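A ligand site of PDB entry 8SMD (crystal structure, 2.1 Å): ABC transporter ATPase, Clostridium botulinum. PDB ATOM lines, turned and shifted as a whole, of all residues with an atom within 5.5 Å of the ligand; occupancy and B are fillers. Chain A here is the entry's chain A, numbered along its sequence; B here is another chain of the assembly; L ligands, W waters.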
ATOM      1  N   PRO A  25      26.653  13.295 -14.415  1.00  0.00           N
ATOM      2  CA  PRO A  25      27.735  12.536 -13.776  1.00  0.00           C
ATOM      3  C   PRO A  25      27.323  11.094 -13.489  1.00  0.00           C
ATOM      4  O   PRO A  25      26.215  10.829 -13.015  1.00  0.00           O
ATOM      5  CB  PRO A  25      27.993  13.317 -12.486  1.00  0.00           C
ATOM      6  CG  PRO A  25      27.556  14.705 -12.800  1.00  0.00           C
ATOM      7  CD  PRO A  25      26.387  14.571 -13.727  1.00  0.00           C
ATOM      8  N   GLY A  26      28.228  10.167 -13.789  1.00  0.00           N
ATOM      9  CA  GLY A  26      27.958   8.755 -13.629  1.00  0.00           C
ATOM     10  C   GLY A  26      26.983   8.164 -14.628  1.00  0.00           C
ATOM     11  O   GLY A  26      26.673   6.975 -14.529  1.00  0.00           O
ATOM     12  N   GLY A  27      26.496   8.956 -15.583  1.00  0.00           N
ATOM     13  CA  GLY A  27      25.550   8.465 -16.558  1.00  0.00           C
ATOM     14  C   GLY A  27      24.105   8.456 -16.108  1.00  0.00           C
ATOM     15  O   GLY A  27      23.272   7.818 -16.770  1.00  0.00           O
ATOM     16  N   HIS A  30      19.559  13.634 -13.157  1.00  0.00           N
ATOM     17  CA  HIS A  30      19.555  14.276 -11.850  1.00  0.00           C
ATOM     18  C   HIS A  30      18.329  15.147 -11.612  1.00  0.00           C
ATOM     19  O   HIS A  30      18.310  15.926 -10.655  1.00  0.00           O
ATOM     20  CB  HIS A  30      20.830  15.116 -11.680  1.00  0.00           C
ATOM     21  CG  HIS A  30      22.075  14.300 -11.537  1.00  0.00           C
ATOM     22  ND1 HIS A  30      22.670  13.660 -12.602  1.00  0.00           N
ATOM     23  CD2 HIS A  30      22.838  14.015 -10.453  1.00  0.00           C
ATOM     24  CE1 HIS A  30      23.741  13.016 -12.184  1.00  0.00           C
ATOM     25  NE2 HIS A  30      23.863  13.217 -10.877  1.00  0.00           N
ATOM     26  N   PHE A  53      18.431  16.252  -7.689  1.00  0.00           N
ATOM     27  CA  PHE A  53      19.447  15.478  -6.993  1.00  0.00           C
ATOM     28  C   PHE A  53      20.774  16.222  -6.946  1.00  0.00           C
ATOM     29  O   PHE A  53      21.050  17.111  -7.754  1.00  0.00           O
ATOM     30  CB  PHE A  53      19.648  14.115  -7.660  1.00  0.00           C
ATOM     31  CG  PHE A  53      18.584  13.117  -7.336  1.00  0.00           C
ATOM     32  CD1 PHE A  53      18.705  12.291  -6.232  1.00  0.00           C
ATOM     33  CD2 PHE A  53      17.465  12.996  -8.130  1.00  0.00           C
ATOM     34  CE1 PHE A  53      17.717  11.362  -5.928  1.00  0.00           C
ATOM     35  CE2 PHE A  53      16.481  12.073  -7.838  1.00  0.00           C
ATOM     36  CZ  PHE A  53      16.607  11.256  -6.737  1.00  0.00           C
ATOM     37  N   GLN A  54      21.605  15.847  -5.970  1.00  0.00           N
ATOM     38  CA  GLN A  54      22.973  16.332  -5.895  1.00  0.00           C
ATOM     39  C   GLN A  54      23.731  15.951  -7.161  1.00  0.00           C
ATOM     40  O   GLN A  54      24.082  14.789  -7.349  1.00  0.00           O
ATOM     41  CB  GLN A  54      23.680  15.756  -4.654  1.00  0.00           C
ATOM     42  CG  GLN A  54      25.176  16.012  -4.595  1.00  0.00           C
ATOM     43  CD  GLN A  54      25.534  17.239  -3.795  1.00  0.00           C
ATOM     44  OE1 GLN A  54      24.699  17.790  -3.072  1.00  0.00           O
ATOM     45  NE2 GLN A  54      26.779  17.676  -3.905  1.00  0.00           N
ATOM     46  N   LYS A  55      23.958  16.920  -8.040  1.00  0.00           N
ATOM     47  CA  LYS A  55      24.686  16.696  -9.293  1.00  0.00           C
ATOM     48  C   LYS A  55      26.136  17.114  -9.084  1.00  0.00           C
ATOM     49  O   LYS A  55      26.423  18.299  -8.907  1.00  0.00           O
ATOM     50  CB  LYS A  55      24.047  17.452 -10.451  1.00  0.00           C
ATOM     51  CG  LYS A  55      24.699  17.134 -11.794  1.00  0.00           C
ATOM     52  CD  LYS A  55      23.758  17.367 -12.959  1.00  0.00           C
ATOM     53  CE  LYS A  55      23.585  18.839 -13.268  1.00  0.00           C
ATOM     54  NZ  LYS A  55      22.774  19.058 -14.495  1.00  0.00           N
ATOM     55  N   GLY A  56      27.036  16.137  -9.102  1.00  0.00           N
ATOM     56  CA  GLY A  56      28.428  16.395  -8.785  1.00  0.00           C
ATOM     57  C   GLY A  56      28.747  15.956  -7.365  1.00  0.00           C
ATOM     58  O   GLY A  56      28.044  16.320  -6.417  1.00  0.00           O
ATOM     59  N   ALA A  57      29.816  15.178  -7.209  1.00  0.00           N
ATOM     60  CA  ALA A  57      30.178  14.648  -5.912  1.00  0.00           C
ATOM     61  C   ALA A  57      30.585  15.772  -4.965  1.00  0.00           C
ATOM     62  O   ALA A  57      30.774  16.923  -5.365  1.00  0.00           O
ATOM     63  CB  ALA A  57      31.284  13.615  -6.051  1.00  0.00           C
ATOM     64  N   ARG A  58      30.736  15.415  -3.677  1.00  0.00           N
ATOM     65  CA  ARG A  58      30.999  16.413  -2.643  1.00  0.00           C
ATOM     66  C   ARG A  58      32.283  17.193  -2.929  1.00  0.00           C
ATOM     67  O   ARG A  58      32.274  18.417  -3.028  1.00  0.00           O
ATOM     68  CB  ARG A  58      31.080  15.748  -1.275  1.00  0.00           C
ATOM     69  CG  ARG A  58      29.743  15.405  -0.648  1.00  0.00           C
ATOM     70  CD  ARG A  58      29.943  14.778   0.721  1.00  0.00           C
ATOM     71  NE  ARG A  58      28.841  13.905   1.097  1.00  0.00           N
ATOM     72  CZ  ARG A  58      28.716  12.642   0.688  1.00  0.00           C
ATOM     73  NH1 ARG A  58      29.614  12.086  -0.119  1.00  0.00           N
ATOM     74  NH2 ARG A  58      27.687  11.920   1.101  1.00  0.00           N
ATOM     75  N   ILE A  68      19.705  13.446  -1.948  1.00  0.00           N
ATOM     76  CA  ILE A  68      20.406  12.209  -2.236  1.00  0.00           C
ATOM     77  C   ILE A  68      19.401  11.065  -2.173  1.00  0.00           C
ATOM     78  O   ILE A  68      18.328  11.185  -1.571  1.00  0.00           O
ATOM     79  CB  ILE A  68      21.591  11.969  -1.272  1.00  0.00           C
ATOM     80  CG1 ILE A  68      22.647  11.067  -1.919  1.00  0.00           C
ATOM     81  CG2 ILE A  68      21.112  11.355   0.033  1.00  0.00           C
ATOM     82  CD1 ILE A  68      23.193  11.616  -3.223  1.00  0.00           C
ATOM     83  N   ASP A  69      19.760   9.952  -2.820  1.00  0.00           N
ATOM     84  CA  ASP A  69      18.809   8.859  -3.017  1.00  0.00           C
ATOM     85  C   ASP A  69      18.380   8.231  -1.697  1.00  0.00           C
ATOM     86  O   ASP A  69      17.229   7.827  -1.539  1.00  0.00           O
ATOM     87  CB  ASP A  69      19.415   7.808  -3.943  1.00  0.00           C
ATOM     88  CG  ASP A  69      20.033   8.410  -5.178  1.00  0.00           C
ATOM     89  OD1 ASP A  69      21.090   9.075  -5.053  1.00  0.00           O
ATOM     90  OD2 ASP A  69      19.468   8.239  -6.284  1.00  0.00           O
ATOM     91  N   ARG A 110      27.869   1.175   0.880  1.00  0.00           N
ATOM     92  CA  ARG A 110      28.631   1.860  -0.172  1.00  0.00           C
ATOM     93  C   ARG A 110      29.257   3.142   0.368  1.00  0.00           C
ATOM     94  O   ARG A 110      30.377   3.495  -0.003  1.00  0.00           O
ATOM     95  CB  ARG A 110      27.721   2.164  -1.358  1.00  0.00           C
ATOM     96  CG  ARG A 110      28.425   2.896  -2.482  1.00  0.00           C
ATOM     97  CD  ARG A 110      27.453   3.319  -3.567  1.00  0.00           C
ATOM     98  NE  ARG A 110      28.121   4.135  -4.578  1.00  0.00           N
ATOM     99  CZ  ARG A 110      28.291   5.443  -4.500  1.00  0.00           C
ATOM    100  NH1 ARG A 110      27.823   6.140  -3.471  1.00  0.00           N
ATOM    101  NH2 ARG A 110      28.951   6.072  -5.468  1.00  0.00           N
ATOM    102  N   ARG A 114      33.328   3.727   0.663  1.00  0.00           N
ATOM    103  CA  ARG A 114      34.002   4.862   0.039  1.00  0.00           C
ATOM    104  C   ARG A 114      34.744   5.722   1.055  1.00  0.00           C
ATOM    105  O   ARG A 114      35.640   6.474   0.671  1.00  0.00           O
ATOM    106  CB  ARG A 114      32.994   5.713  -0.738  1.00  0.00           C
ATOM    107  CG  ARG A 114      32.445   5.029  -1.973  1.00  0.00           C
ATOM    108  CD  ARG A 114      31.580   5.961  -2.795  1.00  0.00           C
ATOM    109  NE  ARG A 114      31.846   5.826  -4.220  1.00  0.00           N
ATOM    110  CZ  ARG A 114      32.723   6.552  -4.897  1.00  0.00           C
ATOM    111  NH1 ARG A 114      33.432   7.489  -4.297  1.00  0.00           N
ATOM    112  NH2 ARG A 114      32.900   6.320  -6.190  1.00  0.00           N
ATOM    113  N   VAL A 119      37.636   7.685  -1.081  1.00  0.00           N
ATOM    114  CA  VAL A 119      37.106   8.097  -2.383  1.00  0.00           C
ATOM    115  C   VAL A 119      35.731   8.721  -2.281  1.00  0.00           C
ATOM    116  O   VAL A 119      35.124   9.025  -3.316  1.00  0.00           O
ATOM    117  CB  VAL A 119      37.087   6.918  -3.371  1.00  0.00           C
ATOM    118  CG1 VAL A 119      38.491   6.348  -3.552  1.00  0.00           C
ATOM    119  CG2 VAL A 119      36.125   5.845  -2.904  1.00  0.00           C
ATOM    120  N   LEU A 120      35.205   8.930  -1.073  1.00  0.00           N
ATOM    121  CA  LEU A 120      33.879   9.516  -0.921  1.00  0.00           C
ATOM    122  C   LEU A 120      33.886  10.950  -1.422  1.00  0.00           C
ATOM    123  O   LEU A 120      34.685  11.777  -0.951  1.00  0.00           O
ATOM    124  CB  LEU A 120      33.434   9.455   0.539  1.00  0.00           C
ATOM    125  CG  LEU A 120      32.016   9.960   0.789  1.00  0.00           C
ATOM    126  CD1 LEU A 120      31.000   9.048   0.106  1.00  0.00           C
ATOM    127  CD2 LEU A 120      31.722  10.083   2.274  1.00  0.00           C
ATOM    128  N   GLY A 121      33.011  11.252  -2.364  1.00  0.00           N
ATOM    129  CA  GLY A 121      32.948  12.581  -2.944  1.00  0.00           C
ATOM    130  C   GLY A 121      33.844  12.812  -4.130  1.00  0.00           C
ATOM    131  O   GLY A 121      34.113  13.972  -4.464  1.00  0.00           O
ATOM    132  N   THR A 122      34.315  11.749  -4.788  1.00  0.00           N
ATOM    133  CA  THR A 122      35.161  11.880  -5.963  1.00  0.00           C
ATOM    134  C   THR A 122      34.568  11.060  -7.099  1.00  0.00           C
ATOM    135  O   THR A 122      33.758  10.160  -6.897  1.00  0.00           O
ATOM    136  CB  THR A 122      36.593  11.410  -5.682  1.00  0.00           C
ATOM    137  OG1 THR A 122      36.606   9.993  -5.459  1.00  0.00           O
ATOM    138  CG2 THR A 122      37.166  12.114  -4.455  1.00  0.00           C
ATOM    139  N   ASN A 123      34.986  11.398  -8.323  1.00  0.00           N
ATOM    140  CA  ASN A 123      34.532  10.693  -9.520  1.00  0.00           C
ATOM    141  C   ASN A 123      35.391   9.464  -9.788  1.00  0.00           C
ATOM    142  O   ASN A 123      36.072   9.335 -10.803  1.00  0.00           O
ATOM    143  CB  ASN A 123      34.532  11.645 -10.716  1.00  0.00           C
ATOM    144  CG  ASN A 123      33.469  12.712 -10.614  1.00  0.00           C
ATOM    145  OD1 ASN A 123      32.427  12.520  -9.981  1.00  0.00           O
ATOM    146  ND2 ASN A 123      33.708  13.851 -11.250  1.00  0.00           N
ATOM    147  N   THR A 124      35.359   8.537  -8.831  1.00  0.00           N
ATOM    148  CA  THR A 124      36.089   7.274  -8.922  1.00  0.00           C
ATOM    149  C   THR A 124      35.124   6.123  -8.698  1.00  0.00           C
ATOM    150  O   THR A 124      33.979   6.313  -8.274  1.00  0.00           O
ATOM    151  CB  THR A 124      37.237   7.216  -7.917  1.00  0.00           C
ATOM    152  OG1 THR A 124      36.720   7.316  -6.583  1.00  0.00           O
ATOM    153  CG2 THR A 124      38.226   8.350  -8.152  1.00  0.00           C
ATOM    154  N   LEU B  14      24.649  13.774   3.931  1.00  0.00           N
ATOM    155  CA  LEU B  14      24.516  14.990   3.139  1.00  0.00           C
ATOM    156  C   LEU B  14      23.369  15.852   3.645  1.00  0.00           C
ATOM    157  O   LEU B  14      23.559  17.040   3.944  1.00  0.00           O
ATOM    158  CB  LEU B  14      24.304  14.641   1.663  1.00  0.00           C
ATOM    159  CG  LEU B  14      25.521  14.739   0.737  1.00  0.00           C
ATOM    160  CD1 LEU B  14      25.130  14.403  -0.698  1.00  0.00           C
ATOM    161  CD2 LEU B  14      26.142  16.128   0.818  1.00  0.00           C
ATOM    162  N   ARG B  79      17.692   5.681 -10.939  1.00  0.00           N
ATOM    163  CA  ARG B  79      19.033   6.202 -10.659  1.00  0.00           C
ATOM    164  C   ARG B  79      20.049   5.078 -10.542  1.00  0.00           C
ATOM    165  O   ARG B  79      21.136   5.149 -11.126  1.00  0.00           O
ATOM    166  CB  ARG B  79      19.009   7.041  -9.380  1.00  0.00           C
ATOM    167  CG  ARG B  79      18.232   8.339  -9.486  1.00  0.00           C
ATOM    168  CD  ARG B  79      19.163   9.514  -9.740  1.00  0.00           C
ATOM    169  NE  ARG B  79      20.079   9.718  -8.625  1.00  0.00           N
ATOM    170  CZ  ARG B  79      21.078  10.583  -8.626  1.00  0.00           C
ATOM    171  NH1 ARG B  79      21.323  11.349  -9.681  1.00  0.00           N
ATOM    172  NH2 ARG B  79      21.865  10.679  -7.556  1.00  0.00           N
ATOM    173  N   LEU B  80      19.705   4.028  -9.791  1.00  0.00           N
ATOM    174  CA  LEU B  80      20.626   2.915  -9.596  1.00  0.00           C
ATOM    175  C   LEU B  80      20.866   2.158 -10.892  1.00  0.00           C
ATOM    176  O   LEU B  80      21.981   1.679 -11.142  1.00  0.00           O
ATOM    177  CB  LEU B  80      20.099   1.978  -8.513  1.00  0.00           C
ATOM    178  CG  LEU B  80      20.124   2.544  -7.090  1.00  0.00           C
ATOM    179  CD1 LEU B  80      19.398   1.621  -6.139  1.00  0.00           C
ATOM    180  CD2 LEU B  80      21.562   2.770  -6.640  1.00  0.00           C
ATOM    181  N   PHE B  83      23.386   4.285 -12.848  1.00  0.00           N
ATOM    182  CA  PHE B  83      24.718   4.197 -12.256  1.00  0.00           C
ATOM    183  C   PHE B  83      25.358   2.846 -12.561  1.00  0.00           C
ATOM    184  O   PHE B  83      26.562   2.778 -12.876  1.00  0.00           O
ATOM    185  CB  PHE B  83      24.652   4.420 -10.753  1.00  0.00           C
ATOM    186  CG  PHE B  83      24.474   5.862 -10.357  1.00  0.00           C
ATOM    187  CD1 PHE B  83      25.144   6.860 -11.033  1.00  0.00           C
ATOM    188  CD2 PHE B  83      23.635   6.207  -9.307  1.00  0.00           C
ATOM    189  CE1 PHE B  83      24.985   8.184 -10.667  1.00  0.00           C
ATOM    190  CE2 PHE B  83      23.471   7.523  -8.939  1.00  0.00           C
ATOM    191  CZ  PHE B  83      24.148   8.514  -9.625  1.00  0.00           C
ATOM    192  N   PHE B  88      30.788   3.937 -12.839  1.00  0.00           N
ATOM    193  CA  PHE B  88      30.917   3.853 -11.388  1.00  0.00           C
ATOM    194  C   PHE B  88      29.980   2.792 -10.804  1.00  0.00           C
ATOM    195  O   PHE B  88      29.334   3.014  -9.774  1.00  0.00           O
ATOM    196  CB  PHE B  88      30.643   5.215 -10.749  1.00  0.00           C
ATOM    197  CG  PHE B  88      31.556   6.306 -11.252  1.00  0.00           C
ATOM    198  CD1 PHE B  88      32.881   6.035 -11.556  1.00  0.00           C
ATOM    199  CD2 PHE B  88      31.086   7.592 -11.423  1.00  0.00           C
ATOM    200  CE1 PHE B  88      33.721   7.025 -12.023  1.00  0.00           C
ATOM    201  CE2 PHE B  88      31.924   8.597 -11.883  1.00  0.00           C
ATOM    202  CZ  PHE B  88      33.239   8.309 -12.181  1.00  0.00           C
ATOM    203  N   SER B  89      29.903   1.642 -11.445  1.00  0.00           N
ATOM    204  CA  SER B  89      29.107   0.548 -10.922  1.00  0.00           C
ATOM    205  C   SER B  89      29.802  -0.100  -9.735  1.00  0.00           C
ATOM    206  O   SER B  89      31.026  -0.023  -9.576  1.00  0.00           O
ATOM    207  CB  SER B  89      28.835  -0.498 -12.006  1.00  0.00           C
ATOM    208  OG  SER B  89      30.043  -1.096 -12.446  1.00  0.00           O
ATOM    209  N   SER B  90      29.008  -0.746  -8.883  1.00  0.00           N
ATOM    210  CA  SER B  90      29.550  -1.395  -7.689  1.00  0.00           C
ATOM    211  C   SER B  90      28.611  -2.504  -7.250  1.00  0.00           C
ATOM    212  O   SER B  90      27.445  -2.545  -7.636  1.00  0.00           O
ATOM    213  CB  SER B  90      29.758  -0.380  -6.555  1.00  0.00           C
ATOM    214  OG  SER B  90      28.531   0.172  -6.143  1.00  0.00           O
ATOM    215  N   ASN B  93      25.603  -1.168  -5.125  1.00  0.00           N
ATOM    216  CA  ASN B  93      24.474  -0.682  -5.903  1.00  0.00           C
ATOM    217  C   ASN B  93      23.630  -1.840  -6.429  1.00  0.00           C
ATOM    218  O   ASN B  93      22.397  -1.753  -6.477  1.00  0.00           O
ATOM    219  CB  ASN B  93      24.955   0.187  -7.057  1.00  0.00           C
ATOM    220  CG  ASN B  93      25.456   1.541  -6.603  1.00  0.00           C
ATOM    221  OD1 ASN B  93      25.095   2.028  -5.538  1.00  0.00           O
ATOM    222  ND2 ASN B  93      26.304   2.156  -7.416  1.00  0.00           N
HETATM  223  N1  LIG L   1      24.851   7.270  -5.459  1.00  0.00           N
HETATM  224  C1  LIG L   1      25.495   8.371  -5.799  1.00  0.00           C
HETATM  225  O1  LIG L   1      29.738   8.059  -8.005  1.00  0.00           O
HETATM  226  C2  LIG L   1      25.156   6.105  -6.032  1.00  0.00           C
HETATM  227  C3  LIG L   1      26.170   6.071  -6.996  1.00  0.00           C
HETATM  228  C4  LIG L   1      26.818   7.233  -7.329  1.00  0.00           C
HETATM  229  C5  LIG L   1      26.673  11.933  -5.183  1.00  0.00           C
HETATM  230  C6  LIG L   1      26.802  12.536  -6.536  1.00  0.00           C
HETATM  231  C7  LIG L   1      25.918  11.824  -7.515  1.00  0.00           C
HETATM  232  C8  LIG L   1      26.574  12.019  -8.805  1.00  0.00           C
HETATM  233  C9  LIG L   1      28.001  12.316  -8.492  1.00  0.00           C
HETATM  234  C10 LIG L   1      27.654   5.607  -8.505  1.00  0.00           C
HETATM  235  C11 LIG L   1      28.636   7.784  -8.904  1.00  0.00           C
HETATM  236  C12 LIG L   1      27.990   9.120  -9.209  1.00  0.00           C
HETATM  237  C13 LIG L   1      28.626  10.086  -8.321  1.00  0.00           C
HETATM  238  C14 LIG L   1      29.926   9.494  -7.989  1.00  0.00           C
HETATM  239  C15 LIG L   1      30.377   9.953  -6.623  1.00  0.00           C
HETATM  240  N2  LIG L   1      26.454   8.376  -6.708  1.00  0.00           N
HETATM  241  N3  LIG L   1      27.735   6.910  -8.274  1.00  0.00           N
HETATM  242  N4  LIG L   1      26.707   5.083  -7.745  1.00  0.00           N
HETATM  243  N5  LIG L   1      24.447   4.897  -5.657  1.00  0.00           N
HETATM  244  O2  LIG L   1      29.886   9.066  -5.651  1.00  0.00           O
HETATM  245  O3  LIG L   1      25.983  13.135  -9.488  1.00  0.00           O
HETATM  246  O4  LIG L   1      24.621  12.412  -7.525  1.00  0.00           O
HETATM  247  O5  LIG L   1      28.244   9.489 -10.564  1.00  0.00           O
HETATM  248  O6  LIG L   1      28.438   9.146  -3.617  1.00  0.00           O
HETATM  249  O7  LIG L   1      30.776   9.094  -3.170  1.00  0.00           O
HETATM  250  O8  LIG L   1      29.637  11.301  -4.093  1.00  0.00           O
HETATM  251  O9  LIG L   1      27.774  11.123  -2.425  1.00  0.00           O
HETATM  252  O10 LIG L   1      29.039  13.144  -2.302  1.00  0.00           O
HETATM  253  O11 LIG L   1      27.307  12.779  -4.259  1.00  0.00           O
HETATM  254  O12 LIG L   1      28.128  12.342  -7.044  1.00  0.00           O
HETATM  255  O13 LIG L   1      28.824  11.351  -9.019  1.00  0.00           O
HETATM  256  P1  LIG L   1      29.752   9.651  -4.130  1.00  0.00           P
HETATM  257  P2  LIG L   1      28.476  12.152  -3.280  1.00  0.00           P
HETATM  258  O   HOH W   1      22.862   7.886  -3.680  1.00  0.00           O
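O4 of the ligand sits at hydrogen-bond distance from O of Gln 54 (2.4 Å).
The backbone NH (N) of Arg 58 lies close to an oxygen (O10) of the ligand (3.2 Å).
O10 of the ligand lies within salt-bridge range of NH1 of Arg 58 (2.5 Å).
O3 of the ligand lies within hydrogen-bond range of NE2 of His 30 (2.5 Å).
The side-chain amide oxygen (OD1) of Asn 93 of chain B lies within hydrogen-bond range of a nitrogen (N5) of the ligand.
NH1 of Arg 110 is in salt-bridge range of O6 of the ligand (3.1 Å).
The backbone NH of Gly 26 sits close to an oxygen (O5) of the ligand.
N of Gly 56 is in hydrogen-bond range of O3 of the ligand.
N of Gly 121 lies within hydrogen-bond range of O7 of the ligand (3.2 Å).
O4 of the ligand is in hydrogen-bond range of NH2 of Arg 79 of chain B.
The guanidinium group (NH1) of Arg 114 is in salt-bridge range of an oxygen (O7) of the ligand.
N of Ala 57 sits close to O12 of the ligand, at 3.3 Å.
An oxygen (O5) of the ligand lies within hydrogen-bond range of the backbone carbonyl oxygen of Pro 25, at 3.5 Å.
Water W1 bridges OD1 of Asp 69 and N1 of the ligand.
O of Gly 56 lies within hydrogen-bond range of NE2 of Gln 54 (3.1 Å).
NH1 of Arg 79 of chain B sits close to NE2 of His 30, 3.4 Å away.
The backbone carbonyl oxygen (O) of His 30 lies within hydrogen-bond range of the backbone NH (N) of Phe 53 (3.0 Å).
The side-chain amide nitrogen (ND2) of Asn 93 of chain B is in hydrogen-bond range of the side-chain hydroxyl (OG) of Ser 90 of chain B, at 3.2 Å.
The guanidinium group of Arg 79 of chain B is in salt-bridge range of the side-chain carboxylate of Asp 69, 2.8 Å away.
O of Arg 114 sits at hydrogen-bond distance from N of Leu 120.
OG1 of Thr 122 lies within hydrogen-bond range of O of Val 119, at 2.8 Å.
OG1 of Thr 124 sits at hydrogen-bond distance from OG1 of Thr 122 (2.9 Å).
CA of Lys 55 touches O3 of the ligand, at 3.8 Å.
Leu 120 touches the ligand.
Thr 122 touches the ligand.
Asn 123 touches the ligand.
CD2 of Leu 80 of chain B touches N5 of the ligand, 3.7 Å away.
Phe 83 of chain B touches the ligand.
Phe 88 of chain B touches the ligand.
Within 4 Å of the ligand: Pro 25, Gly 26, His 30, Gln 54, Lys 55, Gly 56, Ala 57, Arg 58, Arg 110, Arg 114, Leu 120, Gly 121, Thr 122, Asn 123, Arg 79 of chain B, Leu 80 of chain B, Phe 83 of chain B, Phe 88 of chain B and Asn 93 of chain B.
The nearest printed residue that does not touch the ligand is Ile 68 (4.01 Å).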
